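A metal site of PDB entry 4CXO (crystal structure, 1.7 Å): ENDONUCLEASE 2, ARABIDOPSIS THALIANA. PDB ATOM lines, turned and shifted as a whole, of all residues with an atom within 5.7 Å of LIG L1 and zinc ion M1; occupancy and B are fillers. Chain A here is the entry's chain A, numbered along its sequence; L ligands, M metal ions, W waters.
The backbone carbonyl oxygen (O) of Leu 129 lies within hydrogen-bond range of the side-chain hydroxyl (OG) of Ser 132 (2.9 Å). A ring nitrogen (ND1) of His 130 is in hydrogen-bond range of the backbone carbonyl oxygen of His 58. A ring nitrogen (ND1) of His 154 sits at hydrogen-bond distance from the backbone carbonyl oxygen (O) of Gly 138. The backbone NH (N) of Asp 158 sits close to the side-chain amide nitrogen (NE2) of Gln 127 (3.5 Å). The backbone carbonyl oxygen (O) of Lys 137 is in hydrogen-bond range of the side-chain amide nitrogen (ND2) of Asn 140 (2.8 Å). The backbone carbonyl oxygen (O) of His 130 is in hydrogen-bond range of the backbone NH (N) of Ile 60, at 2.7 Å. N of Gly 138 sits at hydrogen-bond distance from O of Tyr 133, 3.0 Å away. The backbone NH (N) of Leu 129 is in hydrogen-bond range of the side-chain amide oxygen (OE1) of Gln 127, 2.9 Å away.
Of the 20 residues printed, 3 come within 4 Å of zinc ion M1.
The backbone carbonyl oxygen of Leu 129 lies close to an oxygen (O7) of LIG L1, 3.3 Å away. Lys 48 touches LIG L1. CB of Tyr 59 touches O7 of LIG L1, at 3.5 Å. Lys 137 touches LIG L1. N of Gly 138 touches O8 of LIG L1, 3.9 Å away. Hydrophobic or aromatic side chains within 4 Å of LIG L1: Tyr 59, His 130 and His 154.
O8 of LIG L1 sits at hydrogen-bond distance from ND2 of Asn 61. The side-chain amide nitrogen of Asn 140 sits at hydrogen-bond distance from an oxygen (O5) of LIG L1, at 2.7 Å.
Zinc ion M1 is bound by O6 of LIG L1 (2.1 Å), O3 of LG2 L2 (2.1 Å), NE2 of His 154 (2.2 Å), NE2 of His 130 (2.2 Å), OD2 of Asp 158 (2.2 Å) and OD1 of Asp 158 (2.5 Å). Zinc ion M1 has six donor atoms within binding distance.
Water W2 lies within hydrogen-bond range of an oxygen (O1) of LIG L1 and the side-chain hydroxyl (OG) of Ser 55. Water W1 lies within hydrogen-bond range of a nitrogen (N2) of LIG L1 (2.8 Å), the backbone carbonyl oxygen (O) of Ile 60 (2.9 Å), the backbone carbonyl oxygen (O) of Leu 129 (3.1 Å), the side-chain amide nitrogen (ND2) of Asn 61 (3.3 Å) and the side-chain hydroxyl (OG) of Ser 132 (3.5 Å).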
ATOM      1  N   TRP A   1     -21.020  11.922  15.326  1.00  0.00           N
ATOM      2  CA  TRP A   1     -20.175  10.726  15.502  1.00  0.00           C
ATOM      3  C   TRP A   1     -18.892  11.037  16.198  1.00  0.00           C
ATOM      4  O   TRP A   1     -18.465  12.169  16.231  1.00  0.00           O
ATOM      5  CB  TRP A   1     -19.806  10.132  14.147  1.00  0.00           C
ATOM      6  CG  TRP A   1     -20.955   9.842  13.220  1.00  0.00           C
ATOM      7  CD1 TRP A   1     -21.367  10.621  12.188  1.00  0.00           C
ATOM      8  CD2 TRP A   1     -21.744   8.675  13.187  1.00  0.00           C
ATOM      9  NE1 TRP A   1     -22.400  10.031  11.528  1.00  0.00           N
ATOM     10  CE2 TRP A   1     -22.664   8.824  12.118  1.00  0.00           C
ATOM     11  CE3 TRP A   1     -21.811   7.530  13.978  1.00  0.00           C
ATOM     12  CZ2 TRP A   1     -23.621   7.861  11.815  1.00  0.00           C
ATOM     13  CZ3 TRP A   1     -22.761   6.551  13.673  1.00  0.00           C
ATOM     14  CH2 TRP A   1     -23.656   6.730  12.592  1.00  0.00           C
ATOM     15  N   LYS A  48     -15.843  23.547  19.325  1.00  0.00           N
ATOM     16  CA  LYS A  48     -17.109  23.773  19.990  1.00  0.00           C
ATOM     17  C   LYS A  48     -17.036  24.792  21.104  1.00  0.00           C
ATOM     18  O   LYS A  48     -18.031  25.455  21.384  1.00  0.00           O
ATOM     19  CB  LYS A  48     -17.667  22.482  20.593  1.00  0.00           C
ATOM     20  CG  LYS A  48     -18.239  21.520  19.593  1.00  0.00           C
ATOM     21  CD  LYS A  48     -18.733  20.282  20.325  1.00  0.00           C
ATOM     22  CE  LYS A  48     -19.276  19.273  19.354  1.00  0.00           C
ATOM     23  NZ  LYS A  48     -20.028  18.201  20.029  1.00  0.00           N
ATOM     24  N   SER A  55     -21.633  25.234  18.681  1.00  0.00           N
ATOM     25  CA  SER A  55     -21.976  23.999  19.388  1.00  0.00           C
ATOM     26  C   SER A  55     -23.343  23.423  18.968  1.00  0.00           C
ATOM     27  O   SER A  55     -23.458  22.222  18.710  1.00  0.00           O
ATOM     28  CB  SER A  55     -21.927  24.229  20.893  1.00  0.00           C
ATOM     29  OG  SER A  55     -22.229  23.038  21.583  1.00  0.00           O
ATOM     30  N   HIS A  58     -24.151  21.143  15.574  1.00  0.00           N
ATOM     31  CA  HIS A  58     -23.854  19.719  15.379  1.00  0.00           C
ATOM     32  C   HIS A  58     -25.074  18.832  15.363  1.00  0.00           C
ATOM     33  O   HIS A  58     -24.957  17.644  15.006  1.00  0.00           O
ATOM     34  CB  HIS A  58     -22.889  19.225  16.444  1.00  0.00           C
ATOM     35  CG  HIS A  58     -21.529  19.824  16.314  1.00  0.00           C
ATOM     36  ND1 HIS A  58     -20.441  19.070  15.959  1.00  0.00           N
ATOM     37  CD2 HIS A  58     -21.089  21.092  16.448  1.00  0.00           C
ATOM     38  CE1 HIS A  58     -19.373  19.849  15.897  1.00  0.00           C
ATOM     39  NE2 HIS A  58     -19.743  21.079  16.195  1.00  0.00           N
ATOM     40  N   TYR A  59     -26.224  19.369  15.732  1.00  0.00           N
ATOM     41  CA  TYR A  59     -27.400  18.524  15.929  1.00  0.00           C
ATOM     42  C   TYR A  59     -28.716  19.250  15.659  1.00  0.00           C
ATOM     43  O   TYR A  59     -28.741  20.443  15.344  1.00  0.00           O
ATOM     44  CB  TYR A  59     -27.389  17.928  17.341  1.00  0.00           C
ATOM     45  CG  TYR A  59     -27.371  18.965  18.438  1.00  0.00           C
ATOM     46  CD1 TYR A  59     -28.543  19.581  18.853  1.00  0.00           C
ATOM     47  CD2 TYR A  59     -26.191  19.325  19.058  1.00  0.00           C
ATOM     48  CE1 TYR A  59     -28.540  20.558  19.831  1.00  0.00           C
ATOM     49  CE2 TYR A  59     -26.169  20.295  20.042  1.00  0.00           C
ATOM     50  CZ  TYR A  59     -27.347  20.901  20.428  1.00  0.00           C
ATOM     51  OH  TYR A  59     -27.336  21.857  21.395  1.00  0.00           O
ATOM     52  N   ILE A  60     -29.801  18.488  15.791  1.00  0.00           N
ATOM     53  CA  ILE A  60     -31.175  18.984  15.715  1.00  0.00           C
ATOM     54  C   ILE A  60     -31.929  18.367  16.857  1.00  0.00           C
ATOM     55  O   ILE A  60     -31.779  17.176  17.122  1.00  0.00           O
ATOM     56  CB  ILE A  60     -31.857  18.539  14.403  1.00  0.00           C
ATOM     57  CG1 ILE A  60     -31.259  19.280  13.219  1.00  0.00           C
ATOM     58  CG2 ILE A  60     -33.352  18.776  14.447  1.00  0.00           C
ATOM     59  CD1 ILE A  60     -31.592  18.708  11.853  1.00  0.00           C
ATOM     60  N   ASN A  61     -32.752  19.169  17.532  1.00  0.00           N
ATOM     61  CA  ASN A  61     -33.695  18.664  18.518  1.00  0.00           C
ATOM     62  C   ASN A  61     -35.101  18.730  17.970  1.00  0.00           C
ATOM     63  O   ASN A  61     -35.504  19.728  17.371  1.00  0.00           O
ATOM     64  CB  ASN A  61     -33.646  19.495  19.797  1.00  0.00           C
ATOM     65  CG  ASN A  61     -32.401  19.245  20.636  1.00  0.00           C
ATOM     66  OD1 ASN A  61     -31.959  20.133  21.348  1.00  0.00           O
ATOM     67  ND2 ASN A  61     -31.856  18.043  20.576  1.00  0.00           N
ATOM     68  N   ASP A 124     -22.421  14.379  10.853  1.00  0.00           N
ATOM     69  CA  ASP A 124     -23.285  14.454  12.034  1.00  0.00           C
ATOM     70  C   ASP A 124     -24.766  14.357  11.732  1.00  0.00           C
ATOM     71  O   ASP A 124     -25.503  13.720  12.486  1.00  0.00           O
ATOM     72  CB  ASP A 124     -22.999  15.731  12.836  1.00  0.00           C
ATOM     73  CG  ASP A 124     -21.882  15.541  13.831  1.00  0.00           C
ATOM     74  OD1 ASP A 124     -21.312  14.429  13.887  1.00  0.00           O
ATOM     75  OD2 ASP A 124     -21.591  16.517  14.554  1.00  0.00           O
ATOM     76  N   GLN A 127     -25.978  10.846  11.920  1.00  0.00           N
ATOM     77  CA  GLN A 127     -25.998  10.095  13.171  1.00  0.00           C
ATOM     78  C   GLN A 127     -27.437  10.223  13.658  1.00  0.00           C
ATOM     79  O   GLN A 127     -27.909  11.318  13.899  1.00  0.00           O
ATOM     80  CB  GLN A 127     -24.994  10.682  14.159  1.00  0.00           C
ATOM     81  CG  GLN A 127     -24.415   9.690  15.180  1.00  0.00           C
ATOM     82  CD  GLN A 127     -25.359   9.345  16.332  1.00  0.00           C
ATOM     83  OE1 GLN A 127     -26.455   8.856  16.112  1.00  0.00           O
ATOM     84  NE2 GLN A 127     -24.900   9.554  17.555  1.00  0.00           N
ATOM     85  N   LEU A 129     -29.090   9.899  16.418  1.00  0.00           N
ATOM     86  CA  LEU A 129     -29.363  10.625  17.637  1.00  0.00           C
ATOM     87  C   LEU A 129     -28.897  12.072  17.589  1.00  0.00           C
ATOM     88  O   LEU A 129     -29.108  12.820  18.530  1.00  0.00           O
ATOM     89  CB  LEU A 129     -28.784   9.885  18.844  1.00  0.00           C
ATOM     90  CG  LEU A 129     -29.533   8.621  19.210  1.00  0.00           C
ATOM     91  CD1 LEU A 129     -28.848   7.894  20.369  1.00  0.00           C
ATOM     92  CD2 LEU A 129     -30.975   8.931  19.543  1.00  0.00           C
ATOM     93  N   HIS A 130     -28.300  12.501  16.478  1.00  0.00           N
ATOM     94  CA  HIS A 130     -28.082  13.920  16.249  1.00  0.00           C
ATOM     95  C   HIS A 130     -29.306  14.624  15.663  1.00  0.00           C
ATOM     96  O   HIS A 130     -29.275  15.813  15.448  1.00  0.00           O
ATOM     97  CB  HIS A 130     -26.872  14.130  15.333  1.00  0.00           C
ATOM     98  CG  HIS A 130     -25.579  14.095  16.065  1.00  0.00           C
ATOM     99  ND1 HIS A 130     -24.721  15.170  16.100  1.00  0.00           N
ATOM    100  CD2 HIS A 130     -25.020  13.139  16.836  1.00  0.00           C
ATOM    101  CE1 HIS A 130     -23.681  14.879  16.851  1.00  0.00           C
ATOM    102  NE2 HIS A 130     -23.848  13.657  17.326  1.00  0.00           N
ATOM    103  N   VAL A 131     -30.361  13.863  15.387  1.00  0.00           N
ATOM    104  CA  VAL A 131     -31.665  14.413  15.008  1.00  0.00           C
ATOM    105  C   VAL A 131     -32.696  13.692  15.878  1.00  0.00           C
ATOM    106  O   VAL A 131     -33.317  12.717  15.472  1.00  0.00           O
ATOM    107  CB  VAL A 131     -31.953  14.208  13.523  1.00  0.00           C
ATOM    108  CG1 VAL A 131     -33.230  14.939  13.097  1.00  0.00           C
ATOM    109  CG2 VAL A 131     -30.783  14.674  12.682  1.00  0.00           C
ATOM    110  N   SER A 132     -32.817  14.152  17.112  1.00  0.00           N
ATOM    111  CA  SER A 132     -33.665  13.432  18.066  1.00  0.00           C
ATOM    112  C   SER A 132     -34.085  14.346  19.209  1.00  0.00           C
ATOM    113  O   SER A 132     -33.997  15.565  19.089  1.00  0.00           O
ATOM    114  CB  SER A 132     -32.945  12.166  18.534  1.00  0.00           C
ATOM    115  OG  SER A 132     -31.857  12.492  19.376  1.00  0.00           O
ATOM    116  N   TYR A 133     -34.551  13.770  20.313  1.00  0.00           N
ATOM    117  CA  TYR A 133     -35.371  14.507  21.264  1.00  0.00           C
ATOM    118  C   TYR A 133     -34.629  15.498  22.137  1.00  0.00           C
ATOM    119  O   TYR A 133     -33.623  15.156  22.772  1.00  0.00           O
ATOM    120  CB  TYR A 133     -36.136  13.562  22.178  1.00  0.00           C
ATOM    121  CG  TYR A 133     -37.018  12.554  21.488  1.00  0.00           C
ATOM    122  CD1 TYR A 133     -37.399  12.687  20.152  1.00  0.00           C
ATOM    123  CD2 TYR A 133     -37.499  11.464  22.189  1.00  0.00           C
ATOM    124  CE1 TYR A 133     -38.212  11.766  19.540  1.00  0.00           C
ATOM    125  CE2 TYR A 133     -38.321  10.526  21.585  1.00  0.00           C
ATOM    126  CZ  TYR A 133     -38.674  10.688  20.261  1.00  0.00           C
ATOM    127  OH  TYR A 133     -39.487   9.752  19.668  1.00  0.00           O
ATOM    128  N   ALA A 134     -35.154  16.711  22.216  1.00  0.00           N
ATOM    129  CA  ALA A 134     -34.667  17.686  23.185  1.00  0.00           C
ATOM    130  C   ALA A 134     -34.787  17.129  24.604  1.00  0.00           C
ATOM    131  O   ALA A 134     -33.923  17.365  25.438  1.00  0.00           O
ATOM    132  CB  ALA A 134     -35.447  18.976  23.072  1.00  0.00           C
ATOM    133  N   LYS A 137     -31.814  15.123  25.450  1.00  0.00           N
ATOM    134  CA  LYS A 137     -30.604  15.687  24.860  1.00  0.00           C
ATOM    135  C   LYS A 137     -29.987  14.711  23.859  1.00  0.00           C
ATOM    136  O   LYS A 137     -28.795  14.407  23.909  1.00  0.00           O
ATOM    137  CB  LYS A 137     -29.605  16.089  25.957  1.00  0.00           C
ATOM    138  CG  LYS A 137     -30.041  17.299  26.793  1.00  0.00           C
ATOM    139  N   GLY A 138     -30.817  14.235  22.952  1.00  0.00           N
ATOM    140  CA  GLY A 138     -30.373  13.298  21.915  1.00  0.00           C
ATOM    141  C   GLY A 138     -29.792  12.010  22.454  1.00  0.00           C
ATOM    142  O   GLY A 138     -28.843  11.463  21.913  1.00  0.00           O
ATOM    143  N   ASN A 140     -28.383  11.634  25.359  1.00  0.00           N
ATOM    144  CA  ASN A 140     -27.301  11.826  26.293  1.00  0.00           C
ATOM    145  C   ASN A 140     -27.708  11.538  27.745  1.00  0.00           C
ATOM    146  O   ASN A 140     -26.877  11.148  28.540  1.00  0.00           O
ATOM    147  CB  ASN A 140     -26.690  13.219  26.146  1.00  0.00           C
ATOM    148  CG  ASN A 140     -25.667  13.275  25.045  1.00  0.00           C
ATOM    149  OD1 ASN A 140     -24.569  12.734  25.184  1.00  0.00           O
ATOM    150  ND2 ASN A 140     -26.012  13.916  23.936  1.00  0.00           N
ATOM    151  N   HIS A 154     -26.444   8.083  23.506  1.00  0.00           N
ATOM    152  CA  HIS A 154     -25.863   8.907  22.459  1.00  0.00           C
ATOM    153  C   HIS A 154     -24.430   8.451  22.111  1.00  0.00           C
ATOM    154  O   HIS A 154     -24.077   8.293  20.934  1.00  0.00           O
ATOM    155  CB  HIS A 154     -25.887  10.375  22.841  1.00  0.00           C
ATOM    156  CG  HIS A 154     -25.402  11.276  21.761  1.00  0.00           C
ATOM    157  ND1 HIS A 154     -26.250  11.891  20.867  1.00  0.00           N
ATOM    158  CD2 HIS A 154     -24.151  11.575  21.363  1.00  0.00           C
ATOM    159  CE1 HIS A 154     -25.536  12.577  19.991  1.00  0.00           C
ATOM    160  NE2 HIS A 154     -24.257  12.399  20.272  1.00  0.00           N
ATOM    161  N   ASP A 158     -22.517   7.372  18.774  1.00  0.00           N
ATOM    162  CA  ASP A 158     -21.350   8.112  18.290  1.00  0.00           C
ATOM    163  C   ASP A 158     -20.126   7.208  18.081  1.00  0.00           C
ATOM    164  O   ASP A 158     -19.378   7.392  17.111  1.00  0.00           O
ATOM    165  CB  ASP A 158     -20.946   9.215  19.271  1.00  0.00           C
ATOM    166  CG  ASP A 158     -21.629  10.543  19.026  1.00  0.00           C
ATOM    167  OD1 ASP A 158     -22.329  10.744  18.008  1.00  0.00           O
ATOM    168  OD2 ASP A 158     -21.446  11.419  19.890  1.00  0.00           O
HETATM  169  P1  LIG L   1     -22.797  17.607  25.120  1.00  0.00           P
HETATM  170  O1  LIG L   1     -22.874  19.074  24.799  1.00  0.00           O
HETATM  171  O2  LIG L   1     -21.467  17.176  25.680  1.00  0.00           O
HETATM  172  O3  LIG L   1     -24.012  17.044  25.834  1.00  0.00           O
HETATM  173  O4  LIG L   1     -22.848  16.883  23.682  1.00  0.00           O
HETATM  174  C1  LIG L   1     -22.588  15.482  23.629  1.00  0.00           C
HETATM  175  C2  LIG L   1     -22.981  14.909  22.278  1.00  0.00           C
HETATM  176  O5  LIG L   1     -24.387  14.936  22.036  1.00  0.00           O
HETATM  177  C3  LIG L   1     -22.429  15.692  21.111  1.00  0.00           C
HETATM  178  O6  LIG L   1     -22.213  14.701  20.116  1.00  0.00           O
HETATM  179  C4  LIG L   1     -23.526  16.650  20.659  1.00  0.00           C
HETATM  180  C5  LIG L   1     -24.753  15.771  20.912  1.00  0.00           C
HETATM  181  N1  LIG L   1     -26.028  16.407  21.290  1.00  0.00           N
HETATM  182  C6  LIG L   1     -27.220  16.059  20.582  1.00  0.00           C
HETATM  183  O7  LIG L   1     -27.172  15.273  19.601  1.00  0.00           O
HETATM  184  N2  LIG L   1     -28.404  16.584  20.941  1.00  0.00           N
HETATM  185  C7  LIG L   1     -28.502  17.425  21.964  1.00  0.00           C
HETATM  186  O8  LIG L   1     -29.612  17.892  22.273  1.00  0.00           O
HETATM  187  C8  LIG L   1     -27.277  17.797  22.733  1.00  0.00           C
HETATM  188  C9  LIG L   1     -27.312  18.734  23.898  1.00  0.00           C
HETATM  189  C10 LIG L   1     -26.074  17.240  22.349  1.00  0.00           C
HETATM  190  S1  LG2 L   2     -20.064  14.887  17.660  1.00  0.00           S
HETATM  191  O1  LG2 L   2     -18.879  14.718  18.562  1.00  0.00           O
HETATM  192  O2  LG2 L   2     -20.733  16.226  17.971  1.00  0.00           O
HETATM  193  O3  LG2 L   2     -20.920  13.694  17.917  1.00  0.00           O
HETATM  194  O4  LG2 L   2     -19.583  14.946  16.227  1.00  0.00           O
HETATM  195 ZN    ZN M   1     -22.634  12.988  18.987  1.00  0.00          ZN
HETATM  196 ZN    ZN M   2     -19.810  13.540  15.000  1.00  0.00          ZN
HETATM  197 ZN    ZN M   3     -19.955  16.980  15.883  1.00  0.00          ZN
HETATM  198  O   HOH W   1     -30.283  15.590  19.048  1.00  0.00           O
HETATM  199  O   HOH W   2     -23.237  20.530  22.799  1.00  0.00           O
